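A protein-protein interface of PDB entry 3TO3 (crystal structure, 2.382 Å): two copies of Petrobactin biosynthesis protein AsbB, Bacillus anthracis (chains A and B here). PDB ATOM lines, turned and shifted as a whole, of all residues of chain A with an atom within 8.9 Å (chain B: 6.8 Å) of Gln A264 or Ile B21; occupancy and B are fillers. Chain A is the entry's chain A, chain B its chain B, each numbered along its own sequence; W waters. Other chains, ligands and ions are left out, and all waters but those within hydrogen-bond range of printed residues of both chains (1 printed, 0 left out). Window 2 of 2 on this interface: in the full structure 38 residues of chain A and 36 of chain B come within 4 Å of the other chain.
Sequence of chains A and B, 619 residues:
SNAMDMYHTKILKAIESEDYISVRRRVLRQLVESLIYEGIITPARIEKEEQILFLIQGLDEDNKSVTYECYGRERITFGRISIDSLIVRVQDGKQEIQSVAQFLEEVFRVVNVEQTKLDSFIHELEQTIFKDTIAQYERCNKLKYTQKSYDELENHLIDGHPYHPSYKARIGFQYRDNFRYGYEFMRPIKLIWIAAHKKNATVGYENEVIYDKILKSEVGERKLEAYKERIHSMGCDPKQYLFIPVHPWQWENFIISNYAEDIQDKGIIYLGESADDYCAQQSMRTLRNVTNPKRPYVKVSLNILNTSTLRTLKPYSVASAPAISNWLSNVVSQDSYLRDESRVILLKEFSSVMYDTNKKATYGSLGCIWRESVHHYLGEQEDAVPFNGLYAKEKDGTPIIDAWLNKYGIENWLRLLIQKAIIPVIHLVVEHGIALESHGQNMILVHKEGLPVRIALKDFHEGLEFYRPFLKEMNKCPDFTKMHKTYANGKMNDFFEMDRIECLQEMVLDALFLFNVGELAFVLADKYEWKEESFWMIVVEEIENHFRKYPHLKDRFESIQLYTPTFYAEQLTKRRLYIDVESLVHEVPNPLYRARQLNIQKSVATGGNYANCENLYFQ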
ATOM      1  N   CYS A 236     -18.504  -2.578  20.169  1.00  0.00           N
ATOM      2  CA  CYS A 236     -17.085  -2.307  20.375  1.00  0.00           C
ATOM      3  C   CYS A 236     -16.572  -3.194  21.494  1.00  0.00           C
ATOM      4  O   CYS A 236     -17.324  -3.625  22.370  1.00  0.00           O
ATOM      5  CB  CYS A 236     -16.892  -0.841  20.743  1.00  0.00           C
ATOM      6  SG  CYS A 236     -17.310   0.218  19.369  1.00  0.00           S
ATOM      7  N   TYR A 241      -9.837  -0.692  24.889  1.00  0.00           N
ATOM      8  CA  TYR A 241      -9.911   0.706  25.329  1.00  0.00           C
ATOM      9  C   TYR A 241      -9.256   0.993  26.679  1.00  0.00           C
ATOM     10  O   TYR A 241      -9.293   0.164  27.584  1.00  0.00           O
ATOM     11  CB  TYR A 241     -11.378   1.146  25.450  1.00  0.00           C
ATOM     12  CG  TYR A 241     -12.061   1.270  24.122  1.00  0.00           C
ATOM     13  CD1 TYR A 241     -12.648   0.155  23.505  1.00  0.00           C
ATOM     14  CD2 TYR A 241     -12.139   2.497  23.479  1.00  0.00           C
ATOM     15  CE1 TYR A 241     -13.271   0.283  22.267  1.00  0.00           C
ATOM     16  CE2 TYR A 241     -12.759   2.622  22.251  1.00  0.00           C
ATOM     17  CZ  TYR A 241     -13.323   1.521  21.654  1.00  0.00           C
ATOM     18  OH  TYR A 241     -13.946   1.664  20.447  1.00  0.00           O
ATOM     19  N   ILE A 256     -14.455  17.630  21.323  1.00  0.00           N
ATOM     20  CA  ILE A 256     -15.620  17.388  20.456  1.00  0.00           C
ATOM     21  C   ILE A 256     -15.435  17.918  19.033  1.00  0.00           C
ATOM     22  O   ILE A 256     -15.724  17.196  18.083  1.00  0.00           O
ATOM     23  CB  ILE A 256     -16.913  17.951  21.044  1.00  0.00           C
ATOM     24  CG1 ILE A 256     -17.301  17.173  22.290  1.00  0.00           C
ATOM     25  CG2 ILE A 256     -18.025  17.820  20.072  1.00  0.00           C
ATOM     26  CD1 ILE A 256     -18.773  17.289  22.583  1.00  0.00           C
ATOM     27  N   TYR A 259     -11.689  16.262  17.603  1.00  0.00           N
ATOM     28  CA  TYR A 259     -11.707  14.787  17.528  1.00  0.00           C
ATOM     29  C   TYR A 259     -12.878  14.120  16.800  1.00  0.00           C
ATOM     30  O   TYR A 259     -13.175  12.955  17.036  1.00  0.00           O
ATOM     31  CB  TYR A 259     -11.436  14.158  18.874  1.00  0.00           C
ATOM     32  CG  TYR A 259     -10.071  14.504  19.421  1.00  0.00           C
ATOM     33  CD1 TYR A 259      -9.802  15.777  19.914  1.00  0.00           C
ATOM     34  CD2 TYR A 259      -9.050  13.542  19.474  1.00  0.00           C
ATOM     35  CE1 TYR A 259      -8.535  16.091  20.461  1.00  0.00           C
ATOM     36  CE2 TYR A 259      -7.824  13.831  20.002  1.00  0.00           C
ATOM     37  CZ  TYR A 259      -7.560  15.107  20.504  1.00  0.00           C
ATOM     38  OH  TYR A 259      -6.316  15.393  21.023  1.00  0.00           O
ATOM     39  N   ALA A 260     -13.688  14.920  16.127  1.00  0.00           N
ATOM     40  CA  ALA A 260     -14.944  14.440  15.611  1.00  0.00           C
ATOM     41  C   ALA A 260     -14.699  13.103  14.885  1.00  0.00           C
ATOM     42  O   ALA A 260     -15.473  12.146  15.027  1.00  0.00           O
ATOM     43  CB  ALA A 260     -15.548  15.490  14.657  1.00  0.00           C
ATOM     44  N   GLU A 261     -13.605  13.040  14.133  1.00  0.00           N
ATOM     45  CA  GLU A 261     -13.296  11.865  13.342  1.00  0.00           C
ATOM     46  C   GLU A 261     -13.147  10.615  14.231  1.00  0.00           C
ATOM     47  O   GLU A 261     -13.600   9.525  13.858  1.00  0.00           O
ATOM     48  CB  GLU A 261     -12.046  12.094  12.499  1.00  0.00           C
ATOM     49  CG  GLU A 261     -11.333  10.818  12.119  1.00  0.00           C
ATOM     50  CD  GLU A 261      -9.897  11.048  11.626  1.00  0.00           C
ATOM     51  OE1 GLU A 261      -9.348  12.168  11.834  1.00  0.00           O
ATOM     52  OE2 GLU A 261      -9.322  10.093  11.031  1.00  0.00           O
ATOM     53  N   ASP A 262     -12.531  10.795  15.402  1.00  0.00           N
ATOM     54  CA  ASP A 262     -12.324   9.710  16.367  1.00  0.00           C
ATOM     55  C   ASP A 262     -13.637   9.391  17.051  1.00  0.00           C
ATOM     56  O   ASP A 262     -13.885   8.244  17.434  1.00  0.00           O
ATOM     57  CB  ASP A 262     -11.280  10.099  17.441  1.00  0.00           C
ATOM     58  CG  ASP A 262     -10.041  10.812  16.842  1.00  0.00           C
ATOM     59  OD1 ASP A 262      -8.945  10.209  16.779  1.00  0.00           O
ATOM     60  OD2 ASP A 262     -10.161  11.983  16.429  1.00  0.00           O
ATOM     61  N   ILE A 263     -14.489  10.397  17.217  1.00  0.00           N
ATOM     62  CA  ILE A 263     -15.761  10.114  17.840  1.00  0.00           C
ATOM     63  C   ILE A 263     -16.578   9.299  16.860  1.00  0.00           C
ATOM     64  O   ILE A 263     -17.267   8.369  17.266  1.00  0.00           O
ATOM     65  CB  ILE A 263     -16.522  11.392  18.261  1.00  0.00           C
ATOM     66  CG1 ILE A 263     -15.851  12.062  19.466  1.00  0.00           C
ATOM     67  CG2 ILE A 263     -17.984  11.064  18.596  1.00  0.00           C
ATOM     68  CD1 ILE A 263     -16.349  13.476  19.684  1.00  0.00           C
ATOM     69  N   GLN A 264     -16.499   9.621  15.565  1.00  0.00           N
ATOM     70  CA  GLN A 264     -17.351   8.923  14.594  1.00  0.00           C
ATOM     71  C   GLN A 264     -16.939   7.440  14.480  1.00  0.00           C
ATOM     72  O   GLN A 264     -17.786   6.553  14.298  1.00  0.00           O
ATOM     73  CB  GLN A 264     -17.317   9.596  13.218  1.00  0.00           C
ATOM     74  CG  GLN A 264     -17.376   8.622  12.035  1.00  0.00           C
ATOM     75  CD  GLN A 264     -18.806   8.196  11.716  1.00  0.00           C
ATOM     76  OE1 GLN A 264     -19.023   7.192  11.032  1.00  0.00           O
ATOM     77  NE2 GLN A 264     -19.793   8.960  12.210  1.00  0.00           N
ATOM     78  N   ASP A 265     -15.643   7.177  14.556  1.00  0.00           N
ATOM     79  CA  ASP A 265     -15.136   5.813  14.396  1.00  0.00           C
ATOM     80  C   ASP A 265     -14.902   5.069  15.709  1.00  0.00           C
ATOM     81  O   ASP A 265     -14.269   4.021  15.719  1.00  0.00           O
ATOM     82  CB  ASP A 265     -13.952   5.696  13.429  1.00  0.00           C
ATOM     83  CG  ASP A 265     -12.719   6.258  13.986  1.00  0.00           C
ATOM     84  OD1 ASP A 265     -12.708   6.486  15.209  1.00  0.00           O
ATOM     85  OD2 ASP A 265     -11.754   6.473  13.216  1.00  0.00           O
ATOM     86  N   LYS A 266     -15.342   5.669  16.810  1.00  0.00           N
ATOM     87  CA  LYS A 266     -15.219   5.075  18.153  1.00  0.00           C
ATOM     88  C   LYS A 266     -13.770   4.937  18.667  1.00  0.00           C
ATOM     89  O   LYS A 266     -13.504   4.169  19.583  1.00  0.00           O
ATOM     90  CB  LYS A 266     -15.870   3.665  18.212  1.00  0.00           C
ATOM     91  CG  LYS A 266     -17.291   3.515  17.636  1.00  0.00           C
ATOM     92  CD  LYS A 266     -18.185   4.667  18.017  1.00  0.00           C
ATOM     93  CE  LYS A 266     -19.491   4.205  18.686  1.00  0.00           C
ATOM     94  NZ  LYS A 266     -20.110   5.281  19.591  1.00  0.00           N
ATOM     95  N   GLY A 267     -12.845   5.720  18.133  1.00  0.00           N
ATOM     96  CA  GLY A 267     -11.548   5.861  18.769  1.00  0.00           C
ATOM     97  C   GLY A 267     -11.732   6.527  20.125  1.00  0.00           C
ATOM     98  O   GLY A 267     -10.935   6.369  21.032  1.00  0.00           O
ATOM     99  N   ILE A 268     -12.811   7.270  20.257  1.00  0.00           N
ATOM    100  CA  ILE A 268     -13.132   7.954  21.488  1.00  0.00           C
ATOM    101  C   ILE A 268     -14.615   7.764  21.741  1.00  0.00           C
ATOM    102  O   ILE A 268     -15.450   7.940  20.829  1.00  0.00           O
ATOM    103  CB  ILE A 268     -12.797   9.463  21.385  1.00  0.00           C
ATOM    104  CG1 ILE A 268     -11.316   9.693  21.663  1.00  0.00           C
ATOM    105  CG2 ILE A 268     -13.606  10.272  22.386  1.00  0.00           C
ATOM    106  CD1 ILE A 268     -10.934  11.132  21.392  1.00  0.00           C
ATOM    107  N   ILE A 269     -14.949   7.375  22.965  1.00  0.00           N
ATOM    108  CA  ILE A 269     -16.349   7.150  23.308  1.00  0.00           C
ATOM    109  C   ILE A 269     -16.678   7.928  24.554  1.00  0.00           C
ATOM    110  O   ILE A 269     -16.027   7.751  25.587  1.00  0.00           O
ATOM    111  CB  ILE A 269     -16.681   5.633  23.561  1.00  0.00           C
ATOM    112  CG1 ILE A 269     -16.432   4.806  22.290  1.00  0.00           C
ATOM    113  CG2 ILE A 269     -18.144   5.471  24.065  1.00  0.00           C
ATOM    114  CD1 ILE A 269     -16.594   3.268  22.450  1.00  0.00           C
ATOM    115  N   TYR A 355      -4.053   9.790  25.078  1.00  0.00           N
ATOM    116  CA  TYR A 355      -4.465   9.442  23.738  1.00  0.00           C
ATOM    117  C   TYR A 355      -3.696  10.397  22.835  1.00  0.00           C
ATOM    118  O   TYR A 355      -3.893  11.606  22.867  1.00  0.00           O
ATOM    119  CB  TYR A 355      -5.968   9.667  23.608  1.00  0.00           C
ATOM    120  CG  TYR A 355      -6.597   9.257  22.283  1.00  0.00           C
ATOM    121  CD1 TYR A 355      -6.985   7.946  22.051  1.00  0.00           C
ATOM    122  CD2 TYR A 355      -6.837  10.195  21.278  1.00  0.00           C
ATOM    123  CE1 TYR A 355      -7.571   7.568  20.864  1.00  0.00           C
ATOM    124  CE2 TYR A 355      -7.443   9.825  20.085  1.00  0.00           C
ATOM    125  CZ  TYR A 355      -7.813   8.517  19.880  1.00  0.00           C
ATOM    126  OH  TYR A 355      -8.417   8.135  18.691  1.00  0.00           O
ATOM    127  N   ALA B  14     -25.089  13.812  16.432  1.00  0.00           N
ATOM    128  CA  ALA B  14     -24.823  14.295  15.080  1.00  0.00           C
ATOM    129  C   ALA B  14     -23.473  13.800  14.580  1.00  0.00           C
ATOM    130  O   ALA B  14     -23.355  13.354  13.434  1.00  0.00           O
ATOM    131  CB  ALA B  14     -24.885  15.816  15.017  1.00  0.00           C
ATOM    132  N   ILE B  15     -22.453  13.895  15.435  1.00  0.00           N
ATOM    133  CA  ILE B  15     -21.112  13.478  15.037  1.00  0.00           C
ATOM    134  C   ILE B  15     -21.087  11.993  14.768  1.00  0.00           C
ATOM    135  O   ILE B  15     -20.359  11.541  13.885  1.00  0.00           O
ATOM    136  CB  ILE B  15     -20.019  13.749  16.095  1.00  0.00           C
ATOM    137  CG1 ILE B  15     -19.874  15.224  16.348  1.00  0.00           C
ATOM    138  CG2 ILE B  15     -18.684  13.294  15.562  1.00  0.00           C
ATOM    139  CD1 ILE B  15     -19.749  15.973  15.066  1.00  0.00           C
ATOM    140  N   GLU B  16     -21.886  11.243  15.531  1.00  0.00           N
ATOM    141  CA  GLU B  16     -21.863   9.779  15.451  1.00  0.00           C
ATOM    142  C   GLU B  16     -22.737   9.279  14.323  1.00  0.00           C
ATOM    143  O   GLU B  16     -22.869   8.079  14.142  1.00  0.00           O
ATOM    144  CB  GLU B  16     -22.379   9.141  16.749  1.00  0.00           C
ATOM    145  CG  GLU B  16     -21.406   9.068  17.910  1.00  0.00           C
ATOM    146  CD  GLU B  16     -22.134   8.934  19.260  1.00  0.00           C
ATOM    147  OE1 GLU B  16     -23.368   9.139  19.305  1.00  0.00           O
ATOM    148  OE2 GLU B  16     -21.485   8.630  20.286  1.00  0.00           O
ATOM    149  N   SER B  17     -23.389  10.186  13.602  1.00  0.00           N
ATOM    150  CA  SER B  17     -24.421   9.772  12.659  1.00  0.00           C
ATOM    151  C   SER B  17     -23.902   9.669  11.234  1.00  0.00           C
ATOM    152  O   SER B  17     -22.713   9.872  10.975  1.00  0.00           O
ATOM    153  CB  SER B  17     -25.549  10.784  12.657  1.00  0.00           C
ATOM    154  OG  SER B  17     -25.197  11.885  11.832  1.00  0.00           O
ATOM    155  N   GLU B  18     -24.825   9.367  10.321  1.00  0.00           N
ATOM    156  CA  GLU B  18     -24.544   9.277   8.904  1.00  0.00           C
ATOM    157  C   GLU B  18     -24.371  10.652   8.263  1.00  0.00           C
ATOM    158  O   GLU B  18     -23.755  10.763   7.200  1.00  0.00           O
ATOM    159  CB  GLU B  18     -25.680   8.550   8.182  1.00  0.00           C
ATOM    160  CG  GLU B  18     -25.827   7.074   8.565  1.00  0.00           C
ATOM    161  CD  GLU B  18     -25.191   6.113   7.552  1.00  0.00           C
ATOM    162  OE1 GLU B  18     -25.574   4.923   7.552  1.00  0.00           O
ATOM    163  OE2 GLU B  18     -24.313   6.542   6.759  1.00  0.00           O
ATOM    164  N   ASP B  19     -24.955  11.689   8.862  1.00  0.00           N
ATOM    165  CA  ASP B  19     -24.825  13.031   8.293  1.00  0.00           C
ATOM    166  C   ASP B  19     -23.374  13.506   8.385  1.00  0.00           C
ATOM    167  O   ASP B  19     -22.900  14.290   7.563  1.00  0.00           O
ATOM    168  CB  ASP B  19     -25.751  14.006   8.995  1.00  0.00           C
ATOM    169  CG  ASP B  19     -27.215  13.744   8.678  1.00  0.00           C
ATOM    170  OD1 ASP B  19     -27.616  14.020   7.536  1.00  0.00           O
ATOM    171  OD2 ASP B  19     -27.962  13.269   9.566  1.00  0.00           O
ATOM    172  N   TYR B  20     -22.663  12.998   9.378  1.00  0.00           N
ATOM    173  CA  TYR B  20     -21.253  13.278   9.455  1.00  0.00           C
ATOM    174  C   TYR B  20     -20.504  12.749   8.201  1.00  0.00           C
ATOM    175  O   TYR B  20     -19.674  13.454   7.633  1.00  0.00           O
ATOM    176  CB  TYR B  20     -20.665  12.730  10.755  1.00  0.00           C
ATOM    177  CG  TYR B  20     -19.175  12.879  10.787  1.00  0.00           C
ATOM    178  CD1 TYR B  20     -18.593  14.077  11.165  1.00  0.00           C
ATOM    179  CD2 TYR B  20     -18.343  11.830  10.386  1.00  0.00           C
ATOM    180  CE1 TYR B  20     -17.211  14.228  11.173  1.00  0.00           C
ATOM    181  CE2 TYR B  20     -16.967  11.975  10.358  1.00  0.00           C
ATOM    182  CZ  TYR B  20     -16.400  13.175  10.767  1.00  0.00           C
ATOM    183  OH  TYR B  20     -15.024  13.319  10.768  1.00  0.00           O
ATOM    184  N   ILE B  21     -20.806  11.516   7.790  1.00  0.00           N
ATOM    185  CA  ILE B  21     -20.185  10.901   6.622  1.00  0.00           C
ATOM    186  C   ILE B  21     -20.488  11.686   5.346  1.00  0.00           C
ATOM    187  O   ILE B  21     -19.573  11.952   4.554  1.00  0.00           O
ATOM    188  CB  ILE B  21     -20.622   9.449   6.449  1.00  0.00           C
ATOM    189  CG1 ILE B  21     -20.243   8.646   7.689  1.00  0.00           C
ATOM    190  CG2 ILE B  21     -20.027   8.825   5.178  1.00  0.00           C
ATOM    191  CD1 ILE B  21     -18.829   8.140   7.704  1.00  0.00           C
ATOM    192  N   SER B  22     -21.747  12.074   5.147  1.00  0.00           N
ATOM    193  CA  SER B  22     -22.096  12.903   3.974  1.00  0.00           C
ATOM    194  C   SER B  22     -21.370  14.231   3.960  1.00  0.00           C
ATOM    195  O   SER B  22     -20.941  14.670   2.907  1.00  0.00           O
ATOM    196  CB  SER B  22     -23.588  13.207   3.873  1.00  0.00           C
ATOM    197  OG  SER B  22     -24.295  12.402   4.772  1.00  0.00           O
ATOM    198  N   VAL B  23     -21.251  14.884   5.111  1.00  0.00           N
ATOM    199  CA  VAL B  23     -20.618  16.208   5.131  1.00  0.00           C
ATOM    200  C   VAL B  23     -19.151  16.066   4.863  1.00  0.00           C
ATOM    201  O   VAL B  23     -18.574  16.828   4.103  1.00  0.00           O
ATOM    202  CB  VAL B  23     -20.909  16.997   6.422  1.00  0.00           C
ATOM    203  CG1 VAL B  23     -19.977  18.239   6.581  1.00  0.00           C
ATOM    204  CG2 VAL B  23     -22.366  17.443   6.404  1.00  0.00           C
ATOM    205  N   ARG B  24     -18.551  15.053   5.463  1.00  0.00           N
ATOM    206  CA  ARG B  24     -17.130  14.806   5.239  1.00  0.00           C
ATOM    207  C   ARG B  24     -16.894  14.583   3.746  1.00  0.00           C
ATOM    208  O   ARG B  24     -15.966  15.141   3.145  1.00  0.00           O
ATOM    209  CB  ARG B  24     -16.659  13.582   6.017  1.00  0.00           C
ATOM    210  CG  ARG B  24     -15.164  13.379   5.985  1.00  0.00           C
ATOM    211  CD  ARG B  24     -14.841  12.004   6.483  1.00  0.00           C
ATOM    212  NE  ARG B  24     -15.346  10.983   5.570  1.00  0.00           N
ATOM    213  CZ  ARG B  24     -15.558   9.724   5.933  1.00  0.00           C
ATOM    214  NH1 ARG B  24     -15.325   9.339   7.190  1.00  0.00           N
ATOM    215  NH2 ARG B  24     -16.016   8.858   5.048  1.00  0.00           N
ATOM    216  N   ARG B  25     -17.756  13.768   3.153  1.00  0.00           N
ATOM    217  CA  ARG B  25     -17.611  13.438   1.761  1.00  0.00           C
ATOM    218  C   ARG B  25     -17.767  14.695   0.905  1.00  0.00           C
ATOM    219  O   ARG B  25     -17.005  14.903  -0.039  1.00  0.00           O
ATOM    220  CB  ARG B  25     -18.625  12.360   1.355  1.00  0.00           C
ATOM    221  CG  ARG B  25     -18.147  10.982   1.735  1.00  0.00           C
ATOM    222  CD  ARG B  25     -19.277  10.011   1.716  1.00  0.00           C
ATOM    223  NE  ARG B  25     -18.809   8.654   1.954  1.00  0.00           N
ATOM    224  CZ  ARG B  25     -19.595   7.588   1.915  1.00  0.00           C
ATOM    225  NH1 ARG B  25     -20.876   7.745   1.603  1.00  0.00           N
ATOM    226  NH2 ARG B  25     -19.105   6.370   2.166  1.00  0.00           N
ATOM    227  N   ARG B  26     -18.754  15.521   1.240  1.00  0.00           N
ATOM    228  CA  ARG B  26     -18.996  16.736   0.486  1.00  0.00           C
ATOM    229  C   ARG B  26     -17.786  17.685   0.574  1.00  0.00           C
ATOM    230  O   ARG B  26     -17.341  18.240  -0.441  1.00  0.00           O
ATOM    231  CB  ARG B  26     -20.264  17.437   0.960  1.00  0.00           C
ATOM    232  CG  ARG B  26     -20.466  18.807   0.321  1.00  0.00           C
ATOM    233  CD  ARG B  26     -21.556  19.633   0.991  1.00  0.00           C
ATOM    234  NE  ARG B  26     -21.441  21.005   0.520  1.00  0.00           N
ATOM    235  CZ  ARG B  26     -22.172  22.035   0.936  1.00  0.00           C
ATOM    236  NH1 ARG B  26     -23.139  21.870   1.849  1.00  0.00           N
ATOM    237  NH2 ARG B  26     -21.947  23.247   0.414  1.00  0.00           N
ATOM    238  N   GLU B  96     -11.471   4.466   1.328  1.00  0.00           N
ATOM    239  CA  GLU B  96     -12.005   5.806   1.249  1.00  0.00           C
ATOM    240  C   GLU B  96     -11.306   6.632   2.317  1.00  0.00           C
ATOM    241  O   GLU B  96     -11.156   6.181   3.458  1.00  0.00           O
ATOM    242  CB  GLU B  96     -13.501   5.785   1.524  1.00  0.00           C
ATOM    243  CG  GLU B  96     -14.122   7.181   1.714  1.00  0.00           C
ATOM    244  CD  GLU B  96     -15.607   7.136   2.116  1.00  0.00           C
ATOM    245  OE1 GLU B  96     -16.145   8.246   2.313  1.00  0.00           O
ATOM    246  OE2 GLU B  96     -16.221   6.023   2.242  1.00  0.00           O
ATOM    247  N   GLN B  98     -10.652   8.935   5.300  1.00  0.00           N
ATOM    248  CA  GLN B  98     -11.358   9.417   6.492  1.00  0.00           C
ATOM    249  C   GLN B  98     -10.862  10.712   7.142  1.00  0.00           C
ATOM    250  O   GLN B  98     -11.546  11.301   7.986  1.00  0.00           O
ATOM    251  CB  GLN B  98     -11.307   8.337   7.552  1.00  0.00           C
ATOM    252  CG  GLN B  98     -11.313   6.961   6.984  1.00  0.00           C
ATOM    253  CD  GLN B  98     -12.473   6.188   7.501  1.00  0.00           C
ATOM    254  OE1 GLN B  98     -12.298   5.246   8.280  1.00  0.00           O
ATOM    255  NE2 GLN B  98     -13.684   6.604   7.113  1.00  0.00           N
ATOM    256  N   THR B 133     -22.173  19.197   9.889  1.00  0.00           N
ATOM    257  CA  THR B 133     -22.733  17.944  10.390  1.00  0.00           C
ATOM    258  C   THR B 133     -23.897  18.188  11.353  1.00  0.00           C
ATOM    259  O   THR B 133     -24.927  17.553  11.248  1.00  0.00           O
ATOM    260  CB  THR B 133     -21.675  17.092  11.120  1.00  0.00           C
ATOM    261  OG1 THR B 133     -20.701  16.626  10.180  1.00  0.00           O
ATOM    262  CG2 THR B 133     -22.339  15.901  11.816  1.00  0.00           C
HETATM  263  O   HOH W   1     -11.642   7.150  10.533  1.00  0.00           O
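The side-chain hydroxyl (OH) of Tyr A241 lies within hydrogen-bond range of the backbone carbonyl oxygen (O) of Lys A266. The backbone carbonyl oxygen (O) of Ala B14 lies within hydrogen-bond range of the side-chain hydroxyl (OG) of Ser B17 (2.8 Å). The side-chain hydroxyl (OG) of Ser B17 is in hydrogen-bond range of the backbone NH (N) of Asp B19 (3.0 Å). The guanidinium group (NH1) of Arg B24 lies close to the side-chain amide nitrogen (NE2) of Gln B98, 3.2 Å away.
Water W1 bridges OD2 of Asp A265 and OE1 of Gln B98.
Of chain B, only Ile B15 (3.1 Å), Glu B16 (3.6 Å), Ser B17 (3.3 Å), Tyr B20 (3.7 Å) and Ile B21 (3.5 Å) come within 4 Å of Gln A264. No residue of chain A comes within 4 Å of Ser B22. Of the printed residues of chain A, Glu B16 touches Gln A264 and Lys A266. Of the printed residues of chain A, Gln B98 touches Glu A261 (3.96 Å). Printed residues of chain A within 4 Å of Ser B17: Gln A264 (3.3 Å). Of the printed residues of chain A, Ile B15 touches Ala A260 (3.5 Å), Ile A263 (3.8 Å) and Gln A264 (3.1 Å). Of the printed residues of chain B, Ile A263 touches Ile B15 (3.8 Å). Arg B24 touches none of the printed residues of chain A. Val B23 touches none of the printed residues of chain A. The nearest printed residue of chain B that does not touch Ala A260 is Tyr B20 (4.1 Å).
NE2 of Gln A264 lies within hydrogen-bond range of O of Ile B15 (3.1 Å). The backbone carbonyl oxygen (O) of Ser B17 is in hydrogen-bond range of the side-chain amide nitrogen (NE2) of Gln A264 (3.3 Å). The side-chain carboxylate of Glu B16 is in salt-bridge range of the side-chain amino group of Lys A266 (3.7 Å).
Hydrophobic or aromatic side chains of chain A that line the printed part of chain B: Ala A260 and Ile A263. Among the printed residues, Asp or Glu carboxylates within 4 Å of a Lys or Arg side-chain nitrogen of the other chain: Lys A266 with Glu B16 (3.7 Å).
No position is printed for both chains. Of the 10 pairs that touch across the chains among the printed residues, none has its exchanged pair printed and touching as well.
Among the printed residues, pairs that only touch across the chains: Glu A261 with Tyr B20, Ala A260 with Ile B15, Gln A264 with Ile B21, Gln A264 with Glu B16, Gln A264 with Tyr B20, Ile A263 with Ile B15 and Glu A261 with Gln B98.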
